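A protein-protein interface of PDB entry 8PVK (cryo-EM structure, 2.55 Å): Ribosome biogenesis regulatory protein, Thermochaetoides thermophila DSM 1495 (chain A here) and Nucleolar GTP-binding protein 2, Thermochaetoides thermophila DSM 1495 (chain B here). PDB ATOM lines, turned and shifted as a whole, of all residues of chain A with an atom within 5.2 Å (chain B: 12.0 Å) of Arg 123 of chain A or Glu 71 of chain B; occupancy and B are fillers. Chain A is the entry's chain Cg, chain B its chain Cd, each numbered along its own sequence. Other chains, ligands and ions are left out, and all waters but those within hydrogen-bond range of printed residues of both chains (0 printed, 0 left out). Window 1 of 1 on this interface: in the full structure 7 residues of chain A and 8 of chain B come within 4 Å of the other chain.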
ATOM      1  N   ARG A 119     -11.477  16.205 -29.699  1.00  0.00           N
ATOM      2  CA  ARG A 119     -11.541  17.286 -30.675  1.00  0.00           C
ATOM      3  C   ARG A 119     -10.624  18.442 -30.302  1.00  0.00           C
ATOM      4  O   ARG A 119     -10.142  19.155 -31.188  1.00  0.00           O
ATOM      5  CB  ARG A 119     -12.984  17.767 -30.824  1.00  0.00           C
ATOM      6  CG  ARG A 119     -13.950  16.677 -31.261  1.00  0.00           C
ATOM      7  CD  ARG A 119     -15.351  17.223 -31.460  1.00  0.00           C
ATOM      8  NE  ARG A 119     -15.425  18.134 -32.596  1.00  0.00           N
ATOM      9  CZ  ARG A 119     -15.822  17.787 -33.812  1.00  0.00           C
ATOM     10  NH1 ARG A 119     -16.205  16.552 -34.089  1.00  0.00           N
ATOM     11  NH2 ARG A 119     -15.839  18.704 -34.774  1.00  0.00           N
ATOM     12  N   GLU A 120     -10.378  18.645 -29.006  1.00  0.00           N
ATOM     13  CA  GLU A 120      -9.396  19.636 -28.583  1.00  0.00           C
ATOM     14  C   GLU A 120      -7.977  19.159 -28.870  1.00  0.00           C
ATOM     15  O   GLU A 120      -7.100  19.964 -29.206  1.00  0.00           O
ATOM     16  CB  GLU A 120      -9.569  19.943 -27.092  1.00  0.00           C
ATOM     17  CG  GLU A 120      -8.961  21.263 -26.562  1.00  0.00           C
ATOM     18  CD  GLU A 120      -9.138  22.486 -27.464  1.00  0.00           C
ATOM     19  OE1 GLU A 120     -10.183  22.631 -28.138  1.00  0.00           O
ATOM     20  OE2 GLU A 120      -8.209  23.320 -27.496  1.00  0.00           O
ATOM     21  N   GLN A 121      -7.737  17.853 -28.736  1.00  0.00           N
ATOM     22  CA  GLN A 121      -6.409  17.302 -28.992  1.00  0.00           C
ATOM     23  C   GLN A 121      -6.054  17.346 -30.472  1.00  0.00           C
ATOM     24  O   GLN A 121      -4.887  17.557 -30.820  1.00  0.00           O
ATOM     25  CB  GLN A 121      -6.336  15.865 -28.470  1.00  0.00           C
ATOM     26  CG  GLN A 121      -4.978  15.200 -28.592  1.00  0.00           C
ATOM     27  CD  GLN A 121      -5.003  13.746 -28.162  1.00  0.00           C
ATOM     28  OE1 GLN A 121      -6.033  13.233 -27.725  1.00  0.00           O
ATOM     29  NE2 GLN A 121      -3.867  13.072 -28.289  1.00  0.00           N
ATOM     30  N   ARG A 122      -7.035  17.167 -31.355  1.00  0.00           N
ATOM     31  CA  ARG A 122      -6.764  17.097 -32.784  1.00  0.00           C
ATOM     32  C   ARG A 122      -6.914  18.444 -33.494  1.00  0.00           C
ATOM     33  O   ARG A 122      -7.030  18.472 -34.725  1.00  0.00           O
ATOM     34  CB  ARG A 122      -7.662  16.050 -33.443  1.00  0.00           C
ATOM     35  CG  ARG A 122      -9.139  16.387 -33.434  1.00  0.00           C
ATOM     36  CD  ARG A 122      -9.976  15.149 -33.664  1.00  0.00           C
ATOM     37  NE  ARG A 122     -11.328  15.482 -34.091  1.00  0.00           N
ATOM     38  CZ  ARG A 122     -12.337  14.626 -34.109  1.00  0.00           C
ATOM     39  NH1 ARG A 122     -12.187  13.372 -33.714  1.00  0.00           N
ATOM     40  NH2 ARG A 122     -13.529  15.035 -34.533  1.00  0.00           N
ATOM     41  N   ARG A 123      -6.902  19.553 -32.757  1.00  0.00           N
ATOM     42  CA  ARG A 123      -7.036  20.864 -33.379  1.00  0.00           C
ATOM     43  C   ARG A 123      -5.789  21.231 -34.177  1.00  0.00           C
ATOM     44  O   ARG A 123      -4.668  20.844 -33.839  1.00  0.00           O
ATOM     45  CB  ARG A 123      -7.296  21.941 -32.325  1.00  0.00           C
ATOM     46  CG  ARG A 123      -8.736  22.034 -31.870  1.00  0.00           C
ATOM     47  CD  ARG A 123      -8.996  23.330 -31.123  1.00  0.00           C
ATOM     48  NE  ARG A 123      -8.825  24.503 -31.971  1.00  0.00           N
ATOM     49  CZ  ARG A 123      -8.762  25.748 -31.518  1.00  0.00           C
ATOM     50  NH1 ARG A 123      -8.839  26.018 -30.225  1.00  0.00           N
ATOM     51  NH2 ARG A 123      -8.622  26.747 -32.384  1.00  0.00           N
ATOM     52  N   ASN A 124      -6.001  21.994 -35.249  1.00  0.00           N
ATOM     53  CA  ASN A 124      -4.912  22.495 -36.088  1.00  0.00           C
ATOM     54  C   ASN A 124      -4.406  23.820 -35.515  1.00  0.00           C
ATOM     55  O   ASN A 124      -4.530  24.893 -36.108  1.00  0.00           O
ATOM     56  CB  ASN A 124      -5.379  22.643 -37.531  1.00  0.00           C
ATOM     57  CG  ASN A 124      -4.246  22.961 -38.485  1.00  0.00           C
ATOM     58  OD1 ASN A 124      -3.074  22.789 -38.156  1.00  0.00           O
ATOM     59  ND2 ASN A 124      -4.592  23.433 -39.676  1.00  0.00           N
ATOM     60  N   LEU A 125      -3.827  23.722 -34.322  1.00  0.00           N
ATOM     61  CA  LEU A 125      -3.352  24.899 -33.611  1.00  0.00           C
ATOM     62  C   LEU A 125      -2.306  24.476 -32.594  1.00  0.00           C
ATOM     63  O   LEU A 125      -2.489  23.488 -31.880  1.00  0.00           O
ATOM     64  CB  LEU A 125      -4.503  25.630 -32.910  1.00  0.00           C
ATOM     65  CG  LEU A 125      -4.226  27.072 -32.486  1.00  0.00           C
ATOM     66  CD1 LEU A 125      -3.996  27.963 -33.698  1.00  0.00           C
ATOM     67  CD2 LEU A 125      -5.365  27.598 -31.637  1.00  0.00           C
ATOM     68  N   TRP A 134       0.718  31.938 -32.131  1.00  0.00           N
ATOM     69  CA  TRP A 134      -0.064  30.742 -32.409  1.00  0.00           C
ATOM     70  C   TRP A 134       0.022  30.423 -33.895  1.00  0.00           C
ATOM     71  O   TRP A 134      -0.197  31.300 -34.737  1.00  0.00           O
ATOM     72  CB  TRP A 134      -1.522  30.929 -31.988  1.00  0.00           C
ATOM     73  CG  TRP A 134      -1.708  30.932 -30.507  1.00  0.00           C
ATOM     74  CD1 TRP A 134      -1.702  32.017 -29.682  1.00  0.00           C
ATOM     75  CD2 TRP A 134      -1.914  29.790 -29.668  1.00  0.00           C
ATOM     76  NE1 TRP A 134      -1.898  31.623 -28.382  1.00  0.00           N
ATOM     77  CE2 TRP A 134      -2.030  30.260 -28.347  1.00  0.00           C
ATOM     78  CE3 TRP A 134      -2.015  28.417 -29.907  1.00  0.00           C
ATOM     79  CZ2 TRP A 134      -2.241  29.406 -27.269  1.00  0.00           C
ATOM     80  CZ3 TRP A 134      -2.224  27.571 -28.836  1.00  0.00           C
ATOM     81  CH2 TRP A 134      -2.336  28.067 -27.532  1.00  0.00           C
ATOM     82  N   LYS A 137      -0.491  23.550 -37.307  1.00  0.00           N
ATOM     83  CA  LYS A 137       0.375  22.386 -37.461  1.00  0.00           C
ATOM     84  C   LYS A 137       0.541  21.995 -38.924  1.00  0.00           C
ATOM     85  O   LYS A 137       1.621  21.547 -39.326  1.00  0.00           O
ATOM     86  CB  LYS A 137      -0.176  21.204 -36.665  1.00  0.00           C
ATOM     87  CG  LYS A 137      -0.396  21.483 -35.191  1.00  0.00           C
ATOM     88  CD  LYS A 137      -1.167  20.347 -34.540  1.00  0.00           C
ATOM     89  CE  LYS A 137      -1.285  20.540 -33.039  1.00  0.00           C
ATOM     90  NZ  LYS A 137      -2.231  19.564 -32.430  1.00  0.00           N
ATOM     91  N   LYS B  67       4.235  25.846 -21.142  1.00  0.00           N
ATOM     92  CA  LYS B  67       3.779  27.168 -21.564  1.00  0.00           C
ATOM     93  C   LYS B  67       2.279  27.238 -21.313  1.00  0.00           C
ATOM     94  O   LYS B  67       1.482  26.676 -22.068  1.00  0.00           O
ATOM     95  CB  LYS B  67       4.115  27.418 -23.030  1.00  0.00           C
ATOM     96  CG  LYS B  67       5.601  27.526 -23.320  1.00  0.00           C
ATOM     97  CD  LYS B  67       6.186  28.786 -22.705  1.00  0.00           C
ATOM     98  CE  LYS B  67       7.661  28.930 -23.037  1.00  0.00           C
ATOM     99  NZ  LYS B  67       8.490  27.907 -22.345  1.00  0.00           N
ATOM    100  N   ALA B  68       1.891  27.930 -20.245  1.00  0.00           N
ATOM    101  CA  ALA B  68       0.485  28.046 -19.862  1.00  0.00           C
ATOM    102  C   ALA B  68      -0.104  29.248 -20.586  1.00  0.00           C
ATOM    103  O   ALA B  68      -0.050  30.382 -20.108  1.00  0.00           O
ATOM    104  CB  ALA B  68       0.348  28.163 -18.350  1.00  0.00           C
ATOM    105  N   VAL B  69      -0.675  28.994 -21.761  1.00  0.00           N
ATOM    106  CA  VAL B  69      -1.186  30.037 -22.639  1.00  0.00           C
ATOM    107  C   VAL B  69      -2.612  29.706 -23.053  1.00  0.00           C
ATOM    108  O   VAL B  69      -3.011  28.539 -23.114  1.00  0.00           O
ATOM    109  CB  VAL B  69      -0.283  30.223 -23.879  1.00  0.00           C
ATOM    110  CG1 VAL B  69       1.051  30.821 -23.483  1.00  0.00           C
ATOM    111  CG2 VAL B  69      -0.044  28.885 -24.549  1.00  0.00           C
ATOM    112  N   ILE B  70      -3.389  30.752 -23.329  1.00  0.00           N
ATOM    113  CA  ILE B  70      -4.769  30.632 -23.790  1.00  0.00           C
ATOM    114  C   ILE B  70      -4.851  31.245 -25.180  1.00  0.00           C
ATOM    115  O   ILE B  70      -4.475  32.408 -25.374  1.00  0.00           O
ATOM    116  CB  ILE B  70      -5.760  31.319 -22.836  1.00  0.00           C
ATOM    117  CG1 ILE B  70      -5.594  30.797 -21.405  1.00  0.00           C
ATOM    118  CG2 ILE B  70      -7.192  31.149 -23.336  1.00  0.00           C
ATOM    119  CD1 ILE B  70      -6.283  29.471 -21.142  1.00  0.00           C
ATOM    120  N   GLU B  71      -5.340  30.470 -26.142  1.00  0.00           N
ATOM    121  CA  GLU B  71      -5.467  30.977 -27.497  1.00  0.00           C
ATOM    122  C   GLU B  71      -6.681  31.896 -27.617  1.00  0.00           C
ATOM    123  O   GLU B  71      -7.642  31.774 -26.852  1.00  0.00           O
ATOM    124  CB  GLU B  71      -5.577  29.818 -28.491  1.00  0.00           C
ATOM    125  CG  GLU B  71      -6.985  29.296 -28.752  1.00  0.00           C
ATOM    126  CD  GLU B  71      -7.446  28.287 -27.715  1.00  0.00           C
ATOM    127  OE1 GLU B  71      -6.678  27.996 -26.774  1.00  0.00           O
ATOM    128  OE2 GLU B  71      -8.579  27.779 -27.846  1.00  0.00           O
ATOM    129  N   PRO B  72      -6.641  32.859 -28.537  1.00  0.00           N
ATOM    130  CA  PRO B  72      -7.852  33.633 -28.826  1.00  0.00           C
ATOM    131  C   PRO B  72      -8.869  32.779 -29.563  1.00  0.00           C
ATOM    132  O   PRO B  72      -8.531  32.025 -30.478  1.00  0.00           O
ATOM    133  CB  PRO B  72      -7.343  34.786 -29.697  1.00  0.00           C
ATOM    134  CG  PRO B  72      -6.060  34.300 -30.266  1.00  0.00           C
ATOM    135  CD  PRO B  72      -5.462  33.390 -29.242  1.00  0.00           C
ATOM    136  N   ASN B  73     -10.127  32.901 -29.151  1.00  0.00           N
ATOM    137  CA  ASN B  73     -11.187  32.071 -29.701  1.00  0.00           C
ATOM    138  C   ASN B  73     -12.513  32.791 -29.517  1.00  0.00           C
ATOM    139  O   ASN B  73     -12.764  33.375 -28.460  1.00  0.00           O
ATOM    140  CB  ASN B  73     -11.226  30.698 -29.020  1.00  0.00           C
ATOM    141  CG  ASN B  73     -11.853  29.630 -29.889  1.00  0.00           C
ATOM    142  OD1 ASN B  73     -12.815  29.883 -30.612  1.00  0.00           O
ATOM    143  ND2 ASN B  73     -11.312  28.421 -29.816  1.00  0.00           N
ATOM    144  N   ARG B  74     -13.356  32.738 -30.550  1.00  0.00           N
ATOM    145  CA  ARG B  74     -14.670  33.363 -30.476  1.00  0.00           C
ATOM    146  C   ARG B  74     -15.604  32.640 -29.515  1.00  0.00           C
ATOM    147  O   ARG B  74     -16.590  33.233 -29.069  1.00  0.00           O
ATOM    148  CB  ARG B  74     -15.302  33.423 -31.866  1.00  0.00           C
ATOM    149  N   LYS B  75     -15.313  31.378 -29.185  1.00  0.00           N
ATOM    150  CA  LYS B  75     -16.177  30.608 -28.299  1.00  0.00           C
ATOM    151  C   LYS B  75     -16.139  31.104 -26.858  1.00  0.00           C
ATOM    152  O   LYS B  75     -17.057  30.795 -26.091  1.00  0.00           O
ATOM    153  CB  LYS B  75     -15.793  29.126 -28.352  1.00  0.00           C
ATOM    154  CG  LYS B  75     -14.536  28.776 -27.571  1.00  0.00           C
ATOM    155  CD  LYS B  75     -14.476  27.297 -27.239  1.00  0.00           C
ATOM    156  CE  LYS B  75     -14.040  26.484 -28.441  1.00  0.00           C
ATOM    157  NZ  LYS B  75     -13.626  25.110 -28.055  1.00  0.00           N
ATOM    158  N   TRP B  76     -15.108  31.862 -26.470  1.00  0.00           N
ATOM    159  CA  TRP B  76     -15.027  32.356 -25.102  1.00  0.00           C
ATOM    160  C   TRP B  76     -16.049  33.447 -24.812  1.00  0.00           C
ATOM    161  O   TRP B  76     -16.378  33.676 -23.645  1.00  0.00           O
ATOM    162  CB  TRP B  76     -13.626  32.900 -24.800  1.00  0.00           C
ATOM    163  CG  TRP B  76     -12.456  31.980 -25.084  1.00  0.00           C
ATOM    164  CD1 TRP B  76     -11.312  32.317 -25.745  1.00  0.00           C
ATOM    165  CD2 TRP B  76     -12.293  30.608 -24.681  1.00  0.00           C
ATOM    166  NE1 TRP B  76     -10.460  31.246 -25.800  1.00  0.00           N
ATOM    167  CE2 TRP B  76     -11.036  30.184 -25.156  1.00  0.00           C
ATOM    168  CE3 TRP B  76     -13.087  29.696 -23.978  1.00  0.00           C
ATOM    169  CZ2 TRP B  76     -10.558  28.892 -24.951  1.00  0.00           C
ATOM    170  CZ3 TRP B  76     -12.611  28.415 -23.779  1.00  0.00           C
ATOM    171  CH2 TRP B  76     -11.358  28.026 -24.263  1.00  0.00           C
ATOM    172  N   PHE B  77     -16.555  34.120 -25.843  1.00  0.00           N
ATOM    173  CA  PHE B  77     -17.414  35.281 -25.669  1.00  0.00           C
ATOM    174  C   PHE B  77     -18.854  35.012 -26.079  1.00  0.00           C
ATOM    175  O   PHE B  77     -19.625  35.959 -26.259  1.00  0.00           O
ATOM    176  CB  PHE B  77     -16.848  36.469 -26.452  1.00  0.00           C
ATOM    177  CG  PHE B  77     -15.437  36.824 -26.072  1.00  0.00           C
ATOM    178  CD1 PHE B  77     -15.188  37.710 -25.038  1.00  0.00           C
ATOM    179  CD2 PHE B  77     -14.359  36.267 -26.745  1.00  0.00           C
ATOM    180  CE1 PHE B  77     -13.894  38.034 -24.681  1.00  0.00           C
ATOM    181  CE2 PHE B  77     -13.065  36.586 -26.390  1.00  0.00           C
ATOM    182  CZ  PHE B  77     -12.832  37.472 -25.360  1.00  0.00           C
ATOM    183  N   THR B  78     -19.234  33.749 -26.229  1.00  0.00           N
ATOM    184  CA  THR B  78     -20.592  33.362 -26.576  1.00  0.00           C
ATOM    185  C   THR B  78     -21.274  32.719 -25.377  1.00  0.00           C
ATOM    186  O   THR B  78     -20.644  32.387 -24.370  1.00  0.00           O
ATOM    187  CB  THR B  78     -20.600  32.399 -27.769  1.00  0.00           C
ATOM    188  OG1 THR B  78     -19.953  31.175 -27.402  1.00  0.00           O
ATOM    189  CG2 THR B  78     -19.880  33.013 -28.956  1.00  0.00           C
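Along chain B the printed residues that touch a printed residue of chain A span positions 69 to 73. Of the 9 printed residues of chain A, 3 touch a printed residue of chain B. Printed residues of chain A that touch a printed residue of chain B: Arg 123, Leu 125 and Trp 134. Among the printed residues, Asp or Glu carboxylates within 4 Å of a Lys or Arg side-chain nitrogen of the other chain: Arg 123 of chain A with Glu 71 of chain B (3.0 Å).
The guanidinium group of Arg 123 of chain A lies within salt-bridge range of the side-chain carboxylate of Glu 71 of chain B, at 3.0 Å. NH1 of Arg 123 of chain A lies close to ND2 of Asn 73 of chain B.
No residue of chain B comes within 4 Å of Asn 124 of chain A. Leu 125 of chain A touches just one residue of chain B: Glu 71. Of the printed residues of chain B, Trp 134 of chain A touches Val 69, Ile 70 and Glu 71. Printed residues of chain A within 4 Å of Val 69 of chain B: Trp 134. Of the printed residues of chain A, Ile 70 of chain B touches Trp 134. Glu 71 of chain B touches three residues of chain A. Lys 75 of chain B touches none of the printed residues of chain A. The nearest residue of chain B that does not touch Arg 123 of chain A is Lys 75 of chain B (5.3 Å). The nearest printed residue of chain A that does not touch Ile 70 of chain B is Leu 125 of chain A (7.4 Å).
Glu 71 of chain B touches Leu 125 of chain A. Val 69 of chain B touches Trp 134 of chain A (CG2 to CZ2, 3.5 Å). Trp 134 of chain A touches Ile 70 of chain B. Glu 71 of chain B touches Trp 134 of chain A (N to CZ2, 3.5 Å).
The side-chain carboxylate (OE2) of Glu 71 of chain B sits at hydrogen-bond distance from the side-chain amide nitrogen (ND2) of Asn 73 of chain B (3.4 Å). The backbone carbonyl oxygen of Glu 71 of chain B lies within hydrogen-bond range of the indole nitrogen of Trp 76 of chain B, at 3.1 Å. The guanidinium group (NH1) of Arg 123 of chain A lies within salt-bridge range of the side-chain carboxylate (OE2) of Glu 120 of chain A. The backbone NH of Lys 75 of chain B lies close to the side-chain amide oxygen of Asn 73 of chain B, at 3.2 Å. The backbone carbonyl oxygen of Arg 123 of chain A is in hydrogen-bond range of the side-chain amino group of Lys 137 of chain A.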
